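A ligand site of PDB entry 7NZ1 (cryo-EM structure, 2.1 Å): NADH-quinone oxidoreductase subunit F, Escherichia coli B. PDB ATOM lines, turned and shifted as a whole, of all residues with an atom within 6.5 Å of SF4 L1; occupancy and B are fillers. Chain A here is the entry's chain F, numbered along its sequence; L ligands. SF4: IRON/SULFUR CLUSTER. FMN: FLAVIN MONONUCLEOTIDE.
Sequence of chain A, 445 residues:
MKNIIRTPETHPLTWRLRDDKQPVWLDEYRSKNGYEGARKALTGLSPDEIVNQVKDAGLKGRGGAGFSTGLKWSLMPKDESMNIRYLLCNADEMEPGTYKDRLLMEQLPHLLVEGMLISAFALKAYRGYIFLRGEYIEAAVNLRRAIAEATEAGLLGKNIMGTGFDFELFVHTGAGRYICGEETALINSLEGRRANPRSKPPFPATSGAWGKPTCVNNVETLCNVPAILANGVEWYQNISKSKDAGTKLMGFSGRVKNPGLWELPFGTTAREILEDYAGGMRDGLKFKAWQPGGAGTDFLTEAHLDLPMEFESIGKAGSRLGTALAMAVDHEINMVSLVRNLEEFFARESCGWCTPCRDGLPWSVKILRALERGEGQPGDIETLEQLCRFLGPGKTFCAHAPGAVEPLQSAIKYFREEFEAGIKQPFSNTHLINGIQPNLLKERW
A sulfur (S3) of SF4 L1 sits close to the backbone NH of Cys 354 (3.4 Å). The side-chain sulfur (SG) of Cys 354 binds an iron atom (FE2) of SF4 L1. An iron atom (FE3) of SF4 L1 is bound by the side-chain sulfur (SG) of Cys 398 (2.3 Å). An iron atom (FE1) of SF4 L1 is bound by the side-chain sulfur (SG) of Cys 357, 2.3 Å away. The backbone NH (N) of Cys 351 sits close to a sulfur (S2) of SF4 L1 (3.4 Å). The side-chain sulfur (SG) of Cys 351 is bound to an iron atom (FE4) of SF4 L1 (2.3 Å). A sulfur (S3) of SF4 L1 sits close to the side-chain hydroxyl (OG) of Ser 350, at 3.2 Å. The backbone NH (N) of Trp 353 lies close to a sulfur (S3) of SF4 L1 (3.5 Å). S3 of SF4 L1 sits close to N of Gly 352 (3.6 Å). ND1 of His 400 sits close to S2 of SF4 L1.
The side-chain sulfur (SG) of Cys 354 sits close to the backbone NH (N) of Phe 397, at 3.5 Å. OG1 of Thr 396 is in hydrogen-bond range of O of Cys 398, 2.9 Å away. The side-chain sulfur of Cys 357 lies close to the side-chain hydroxyl of Ser 350. The side-chain sulfur (SG) of Cys 357 lies close to a ring nitrogen (ND1) of His 400, 3.3 Å away. SG of Cys 351 lies close to N of Trp 353 (3.5 Å). ND2 of Asn 196 lies close to SG of Cys 351. OG of Ser 350 sits close to N of Gly 352, 3.3 Å away. O of Gly 352 lies within hydrogen-bond range of NH1 of Arg 358, at 2.9 Å.
Merely in contact with SF4 L1: Ile 179, Pro 197, Thr 396, Phe 397 and Ala 401. Hydrophobic or aromatic side chains that line SF4 L1: Ile 179, Pro 197, Trp 353, Phe 397, His 400 and Ala 401. Of the 22 residues printed, 13 come within 4 Å of SF4 L1.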
ATOM      1  N   ILE A 179      23.780 -20.500   8.776  1.00  0.00           N
ATOM      2  CA  ILE A 179      23.775 -19.093   9.162  1.00  0.00           C
ATOM      3  C   ILE A 179      25.156 -18.578   9.540  1.00  0.00           C
ATOM      4  O   ILE A 179      25.384 -17.366   9.555  1.00  0.00           O
ATOM      5  CB  ILE A 179      22.754 -18.904  10.313  1.00  0.00           C
ATOM      6  CG1 ILE A 179      22.351 -17.434  10.520  1.00  0.00           C
ATOM      7  CG2 ILE A 179      23.280 -19.483  11.607  1.00  0.00           C
ATOM      8  CD1 ILE A 179      21.882 -16.746   9.262  1.00  0.00           C
ATOM      9  N   ALA A 195      25.662 -18.688  16.835  1.00  0.00           N
ATOM     10  CA  ALA A 195      25.843 -17.895  15.618  1.00  0.00           C
ATOM     11  C   ALA A 195      24.574 -17.101  15.247  1.00  0.00           C
ATOM     12  O   ALA A 195      23.992 -17.273  14.180  1.00  0.00           O
ATOM     13  CB  ALA A 195      26.278 -18.784  14.466  1.00  0.00           C
ATOM     14  N   ASN A 196      24.169 -16.218  16.154  1.00  0.00           N
ATOM     15  CA  ASN A 196      23.187 -15.206  15.796  1.00  0.00           C
ATOM     16  C   ASN A 196      23.842 -14.123  14.947  1.00  0.00           C
ATOM     17  O   ASN A 196      25.020 -13.816  15.120  1.00  0.00           O
ATOM     18  CB  ASN A 196      22.582 -14.557  17.037  1.00  0.00           C
ATOM     19  CG  ASN A 196      21.991 -15.557  17.991  1.00  0.00           C
ATOM     20  OD1 ASN A 196      22.517 -15.778  19.069  1.00  0.00           O
ATOM     21  ND2 ASN A 196      20.889 -16.183  17.584  1.00  0.00           N
ATOM     22  N   PRO A 197      23.105 -13.526  14.014  1.00  0.00           N
ATOM     23  CA  PRO A 197      23.590 -12.318  13.352  1.00  0.00           C
ATOM     24  C   PRO A 197      23.539 -11.118  14.288  1.00  0.00           C
ATOM     25  O   PRO A 197      22.915 -11.140  15.343  1.00  0.00           O
ATOM     26  CB  PRO A 197      22.630 -12.143  12.171  1.00  0.00           C
ATOM     27  CG  PRO A 197      21.923 -13.440  12.043  1.00  0.00           C
ATOM     28  CD  PRO A 197      21.862 -14.023  13.410  1.00  0.00           C
ATOM     29  N   GLU A 349      17.319 -24.347   9.140  1.00  0.00           N
ATOM     30  CA  GLU A 349      18.563 -23.593   9.251  1.00  0.00           C
ATOM     31  C   GLU A 349      18.382 -22.202   9.845  1.00  0.00           C
ATOM     32  O   GLU A 349      19.337 -21.421   9.842  1.00  0.00           O
ATOM     33  CB  GLU A 349      19.254 -23.487   7.891  1.00  0.00           C
ATOM     34  CG  GLU A 349      19.914 -24.782   7.391  1.00  0.00           C
ATOM     35  CD  GLU A 349      20.895 -25.418   8.382  1.00  0.00           C
ATOM     36  OE1 GLU A 349      21.614 -24.705   9.108  1.00  0.00           O
ATOM     37  OE2 GLU A 349      20.952 -26.668   8.418  1.00  0.00           O
ATOM     38  N   SER A 350      17.174 -21.857  10.304  1.00  0.00           N
ATOM     39  CA  SER A 350      16.947 -20.621  11.028  1.00  0.00           C
ATOM     40  C   SER A 350      17.740 -20.592  12.323  1.00  0.00           C
ATOM     41  O   SER A 350      17.857 -21.608  13.018  1.00  0.00           O
ATOM     42  CB  SER A 350      15.458 -20.453  11.321  1.00  0.00           C
ATOM     43  OG  SER A 350      15.194 -19.256  12.020  1.00  0.00           O
ATOM     44  N   CYS A 351      18.338 -19.448  12.636  1.00  0.00           N
ATOM     45  CA  CYS A 351      19.063 -19.356  13.898  1.00  0.00           C
ATOM     46  C   CYS A 351      18.130 -19.219  15.091  1.00  0.00           C
ATOM     47  O   CYS A 351      18.563 -19.453  16.218  1.00  0.00           O
ATOM     48  CB  CYS A 351      20.060 -18.198  13.847  1.00  0.00           C
ATOM     49  SG  CYS A 351      19.423 -16.612  14.316  1.00  0.00           S
ATOM     50  N   GLY A 352      16.856 -18.875  14.871  1.00  0.00           N
ATOM     51  CA  GLY A 352      15.870 -18.824  15.928  1.00  0.00           C
ATOM     52  C   GLY A 352      15.728 -17.484  16.625  1.00  0.00           C
ATOM     53  O   GLY A 352      14.936 -17.392  17.561  1.00  0.00           O
ATOM     54  N   TRP A 353      16.479 -16.462  16.206  1.00  0.00           N
ATOM     55  CA  TRP A 353      16.450 -15.169  16.886  1.00  0.00           C
ATOM     56  C   TRP A 353      15.134 -14.427  16.669  1.00  0.00           C
ATOM     57  O   TRP A 353      14.499 -13.974  17.627  1.00  0.00           O
ATOM     58  CB  TRP A 353      17.632 -14.322  16.421  1.00  0.00           C
ATOM     59  CG  TRP A 353      17.731 -12.971  17.007  1.00  0.00           C
ATOM     60  CD1 TRP A 353      17.471 -11.784  16.389  1.00  0.00           C
ATOM     61  CD2 TRP A 353      18.125 -12.652  18.340  1.00  0.00           C
ATOM     62  NE1 TRP A 353      17.680 -10.742  17.248  1.00  0.00           N
ATOM     63  CE2 TRP A 353      18.085 -11.249  18.452  1.00  0.00           C
ATOM     64  CE3 TRP A 353      18.499 -13.408  19.456  1.00  0.00           C
ATOM     65  CZ2 TRP A 353      18.407 -10.593  19.641  1.00  0.00           C
ATOM     66  CZ3 TRP A 353      18.823 -12.750  20.620  1.00  0.00           C
ATOM     67  CH2 TRP A 353      18.780 -11.355  20.705  1.00  0.00           C
ATOM     68  N   CYS A 354      14.706 -14.273  15.417  1.00  0.00           N
ATOM     69  CA  CYS A 354      13.579 -13.393  15.115  1.00  0.00           C
ATOM     70  C   CYS A 354      12.334 -14.186  14.721  1.00  0.00           C
ATOM     71  O   CYS A 354      12.418 -15.200  14.026  1.00  0.00           O
ATOM     72  CB  CYS A 354      13.947 -12.358  14.055  1.00  0.00           C
ATOM     73  SG  CYS A 354      14.053 -12.899  12.356  1.00  0.00           S
ATOM     74  N   THR A 355      11.189 -13.712  15.223  1.00  0.00           N
ATOM     75  CA  THR A 355       9.869 -14.342  15.050  1.00  0.00           C
ATOM     76  C   THR A 355       9.451 -14.677  13.612  1.00  0.00           C
ATOM     77  O   THR A 355       8.998 -15.820  13.412  1.00  0.00           O
ATOM     78  CB  THR A 355       8.812 -13.462  15.736  1.00  0.00           C
ATOM     79  OG1 THR A 355       9.227 -13.140  17.073  1.00  0.00           O
ATOM     80  CG2 THR A 355       7.470 -14.174  15.800  1.00  0.00           C
ATOM     81  N   PRO A 356       9.534 -13.795  12.592  1.00  0.00           N
ATOM     82  CA  PRO A 356       8.992 -14.179  11.275  1.00  0.00           C
ATOM     83  C   PRO A 356       9.807 -15.240  10.547  1.00  0.00           C
ATOM     84  O   PRO A 356       9.272 -15.878   9.636  1.00  0.00           O
ATOM     85  CB  PRO A 356       8.997 -12.860  10.484  1.00  0.00           C
ATOM     86  CG  PRO A 356       9.240 -11.804  11.477  1.00  0.00           C
ATOM     87  CD  PRO A 356      10.110 -12.434  12.476  1.00  0.00           C
ATOM     88  N   CYS A 357      11.044 -15.461  10.949  1.00  0.00           N
ATOM     89  CA  CYS A 357      11.835 -16.564  10.429  1.00  0.00           C
ATOM     90  C   CYS A 357      11.616 -17.833  11.236  1.00  0.00           C
ATOM     91  O   CYS A 357      11.358 -18.899  10.667  1.00  0.00           O
ATOM     92  CB  CYS A 357      13.314 -16.188  10.432  1.00  0.00           C
ATOM     93  SG  CYS A 357      14.401 -17.356   9.584  1.00  0.00           S
ATOM     94  N   ARG A 358      11.719 -17.715  12.565  1.00  0.00           N
ATOM     95  CA  ARG A 358      11.577 -18.849  13.472  1.00  0.00           C
ATOM     96  C   ARG A 358      10.193 -19.486  13.410  1.00  0.00           C
ATOM     97  O   ARG A 358      10.063 -20.709  13.451  1.00  0.00           O
ATOM     98  CB  ARG A 358      11.889 -18.390  14.898  1.00  0.00           C
ATOM     99  CG  ARG A 358      11.803 -19.475  15.945  1.00  0.00           C
ATOM    100  CD  ARG A 358      11.889 -19.005  17.411  1.00  0.00           C
ATOM    101  NE  ARG A 358      10.890 -18.001  17.779  1.00  0.00           N
ATOM    102  CZ  ARG A 358      11.107 -16.693  17.808  1.00  0.00           C
ATOM    103  NH1 ARG A 358      12.289 -16.177  17.513  1.00  0.00           N
ATOM    104  NH2 ARG A 358      10.117 -15.880  18.143  1.00  0.00           N
ATOM    105  N   LEU A 361       8.393 -19.406   8.735  1.00  0.00           N
ATOM    106  CA  LEU A 361       8.845 -20.468   7.831  1.00  0.00           C
ATOM    107  C   LEU A 361       8.346 -21.886   8.136  1.00  0.00           C
ATOM    108  O   LEU A 361       8.092 -22.613   7.159  1.00  0.00           O
ATOM    109  CB  LEU A 361      10.376 -20.462   7.720  1.00  0.00           C
ATOM    110  CG  LEU A 361      11.105 -19.375   6.933  1.00  0.00           C
ATOM    111  CD1 LEU A 361      12.597 -19.621   6.962  1.00  0.00           C
ATOM    112  CD2 LEU A 361      10.596 -19.324   5.503  1.00  0.00           C
ATOM    113  N   THR A 396      12.655  -8.906   8.857  1.00  0.00           N
ATOM    114  CA  THR A 396      13.348  -9.860   9.703  1.00  0.00           C
ATOM    115  C   THR A 396      14.714  -9.304  10.085  1.00  0.00           C
ATOM    116  O   THR A 396      15.155  -8.278   9.563  1.00  0.00           O
ATOM    117  CB  THR A 396      13.484 -11.213   9.005  1.00  0.00           C
ATOM    118  OG1 THR A 396      14.166 -11.056   7.756  1.00  0.00           O
ATOM    119  CG2 THR A 396      12.118 -11.792   8.745  1.00  0.00           C
ATOM    120  N   PHE A 397      15.375  -9.995  11.010  1.00  0.00           N
ATOM    121  CA  PHE A 397      16.602  -9.470  11.599  1.00  0.00           C
ATOM    122  C   PHE A 397      17.786  -9.564  10.631  1.00  0.00           C
ATOM    123  O   PHE A 397      18.647  -8.690  10.656  1.00  0.00           O
ATOM    124  CB  PHE A 397      16.925 -10.204  12.904  1.00  0.00           C
ATOM    125  CG  PHE A 397      17.948  -9.503  13.745  1.00  0.00           C
ATOM    126  CD1 PHE A 397      17.610  -8.402  14.519  1.00  0.00           C
ATOM    127  CD2 PHE A 397      19.268  -9.945  13.764  1.00  0.00           C
ATOM    128  CE1 PHE A 397      18.546  -7.761  15.288  1.00  0.00           C
ATOM    129  CE2 PHE A 397      20.218  -9.305  14.539  1.00  0.00           C
ATOM    130  CZ  PHE A 397      19.855  -8.211  15.297  1.00  0.00           C
ATOM    131  N   CYS A 398      17.840 -10.584   9.791  1.00  0.00           N
ATOM    132  CA  CYS A 398      18.909 -10.681   8.805  1.00  0.00           C
ATOM    133  C   CYS A 398      18.286 -11.078   7.460  1.00  0.00           C
ATOM    134  O   CYS A 398      17.070 -11.124   7.307  1.00  0.00           O
ATOM    135  CB  CYS A 398      19.991 -11.664   9.273  1.00  0.00           C
ATOM    136  SG  CYS A 398      19.617 -13.404   9.019  1.00  0.00           S
ATOM    137  N   ALA A 399      19.138 -11.408   6.492  1.00  0.00           N
ATOM    138  CA  ALA A 399      18.692 -11.672   5.125  1.00  0.00           C
ATOM    139  C   ALA A 399      18.356 -13.129   4.842  1.00  0.00           C
ATOM    140  O   ALA A 399      18.063 -13.457   3.685  1.00  0.00           O
ATOM    141  CB  ALA A 399      19.747 -11.192   4.128  1.00  0.00           C
ATOM    142  N   HIS A 400      18.436 -14.013   5.844  1.00  0.00           N
ATOM    143  CA  HIS A 400      18.103 -15.423   5.666  1.00  0.00           C
ATOM    144  C   HIS A 400      16.656 -15.618   5.216  1.00  0.00           C
ATOM    145  O   HIS A 400      16.395 -16.313   4.221  1.00  0.00           O
ATOM    146  CB  HIS A 400      18.351 -16.171   6.965  1.00  0.00           C
ATOM    147  CG  HIS A 400      17.984 -17.615   6.895  1.00  0.00           C
ATOM    148  ND1 HIS A 400      16.924 -18.130   7.602  1.00  0.00           N
ATOM    149  CD2 HIS A 400      18.501 -18.642   6.180  1.00  0.00           C
ATOM    150  CE1 HIS A 400      16.818 -19.419   7.336  1.00  0.00           C
ATOM    151  NE2 HIS A 400      17.761 -19.756   6.478  1.00  0.00           N
ATOM    152  N   ALA A 401      15.706 -15.056   5.966  1.00  0.00           N
ATOM    153  CA  ALA A 401      14.287 -15.173   5.636  1.00  0.00           C
ATOM    154  C   ALA A 401      13.928 -14.558   4.280  1.00  0.00           C
ATOM    155  O   ALA A 401      13.124 -15.187   3.561  1.00  0.00           O
ATOM    156  CB  ALA A 401      13.432 -14.653   6.803  1.00  0.00           C
ATOM    157  N   PRO A 402      14.348 -13.298   3.914  1.00  0.00           N
ATOM    158  CA  PRO A 402      14.106 -12.838   2.525  1.00  0.00           C
ATOM    159  C   PRO A 402      14.637 -13.762   1.430  1.00  0.00           C
ATOM    160  O   PRO A 402      13.997 -13.905   0.393  1.00  0.00           O
ATOM    161  CB  PRO A 402      14.843 -11.494   2.480  1.00  0.00           C
ATOM    162  CG  PRO A 402      14.751 -10.984   3.809  1.00  0.00           C
ATOM    163  CD  PRO A 402      14.906 -12.176   4.703  1.00  0.00           C
HETATM  164 FE1  SF4 L   1      16.190 -16.357  10.621  1.00  0.00          FE
HETATM  165 FE2  SF4 L   1      16.000 -14.057  12.102  1.00  0.00          FE
HETATM  166 FE3  SF4 L   1      18.127 -14.433  10.423  1.00  0.00          FE
HETATM  167 FE4  SF4 L   1      17.913 -15.931  12.720  1.00  0.00          FE
HETATM  168  S1  SF4 L   1      18.192 -13.670  12.578  1.00  0.00           S
HETATM  169  S2  SF4 L   1      18.448 -16.681  10.623  1.00  0.00           S
HETATM  170  S3  SF4 L   1      15.661 -16.200  12.834  1.00  0.00           S
HETATM  171  S4  SF4 L   1      15.929 -14.228   9.832  1.00  0.00           S
HETATM  172  N1  FMN L   2      28.942 -15.505   1.933  1.00  0.00           N
HETATM  173  C2  FMN L   2      29.911 -16.429   1.640  1.00  0.00           C
HETATM  174  O2  FMN L   2      30.960 -16.060   1.123  1.00  0.00           O
HETATM  175  N3  FMN L   2      29.713 -17.755   1.918  1.00  0.00           N
HETATM  176  C4  FMN L   2      28.536 -18.171   2.511  1.00  0.00           C
HETATM  177  O4  FMN L   2      28.373 -19.353   2.755  1.00  0.00           O
HETATM  178  C4A FMN L   2      27.555 -17.233   2.816  1.00  0.00           C
HETATM  179  N5  FMN L   2      26.367 -17.624   3.401  1.00  0.00           N
HETATM  180  C5A FMN L   2      25.396 -16.690   3.699  1.00  0.00           C
HETATM  181  C6  FMN L   2      24.211 -17.109   4.294  1.00  0.00           C
HETATM  182  C7  FMN L   2      23.222 -16.183   4.597  1.00  0.00           C
HETATM  183  C7M FMN L   2      21.961 -16.657   5.238  1.00  0.00           C
HETATM  184  C8  FMN L   2      23.433 -14.838   4.310  1.00  0.00           C
HETATM  185  C8M FMN L   2      22.375 -13.813   4.620  1.00  0.00           C
HETATM  186  C9  FMN L   2      24.611 -14.430   3.713  1.00  0.00           C
HETATM  187  C9A FMN L   2      25.607 -15.345   3.412  1.00  0.00           C
HETATM  188  N10 FMN L   2      26.791 -14.950   2.818  1.00  0.00           N
HETATM  189  C10 FMN L   2      27.754 -15.895   2.519  1.00  0.00           C
HETATM  190  C1' FMN L   2      27.069 -13.496   2.490  1.00  0.00           C
HETATM  191  C2' FMN L   2      27.826 -12.818   3.639  1.00  0.00           C
HETATM  192  O2' FMN L   2      26.943 -12.402   4.650  1.00  0.00           O
HETATM  193  C3' FMN L   2      28.621 -11.618   3.151  1.00  0.00           C
HETATM  194  O3' FMN L   2      27.795 -10.761   2.406  1.00  0.00           O
HETATM  195  C4' FMN L   2      29.829 -12.018   2.317  1.00  0.00           C
HETATM  196  O4' FMN L   2      30.625 -12.963   2.999  1.00  0.00           O
HETATM  197  C5' FMN L   2      30.626 -10.777   2.003  1.00  0.00           C
HETATM  198  O5' FMN L   2      31.844 -11.098   1.382  1.00  0.00           O
HETATM  199  P   FMN L   2      32.095 -10.673  -0.149  1.00  0.00           P
HETATM  200  O1P FMN L   2      32.126  -9.173  -0.241  1.00  0.00           O
HETATM  201  O2P FMN L   2      33.431 -11.196  -0.596  1.00  0.00           O
HETATM  202  O3P FMN L   2      30.998 -11.252  -1.005  1.00  0.00           O
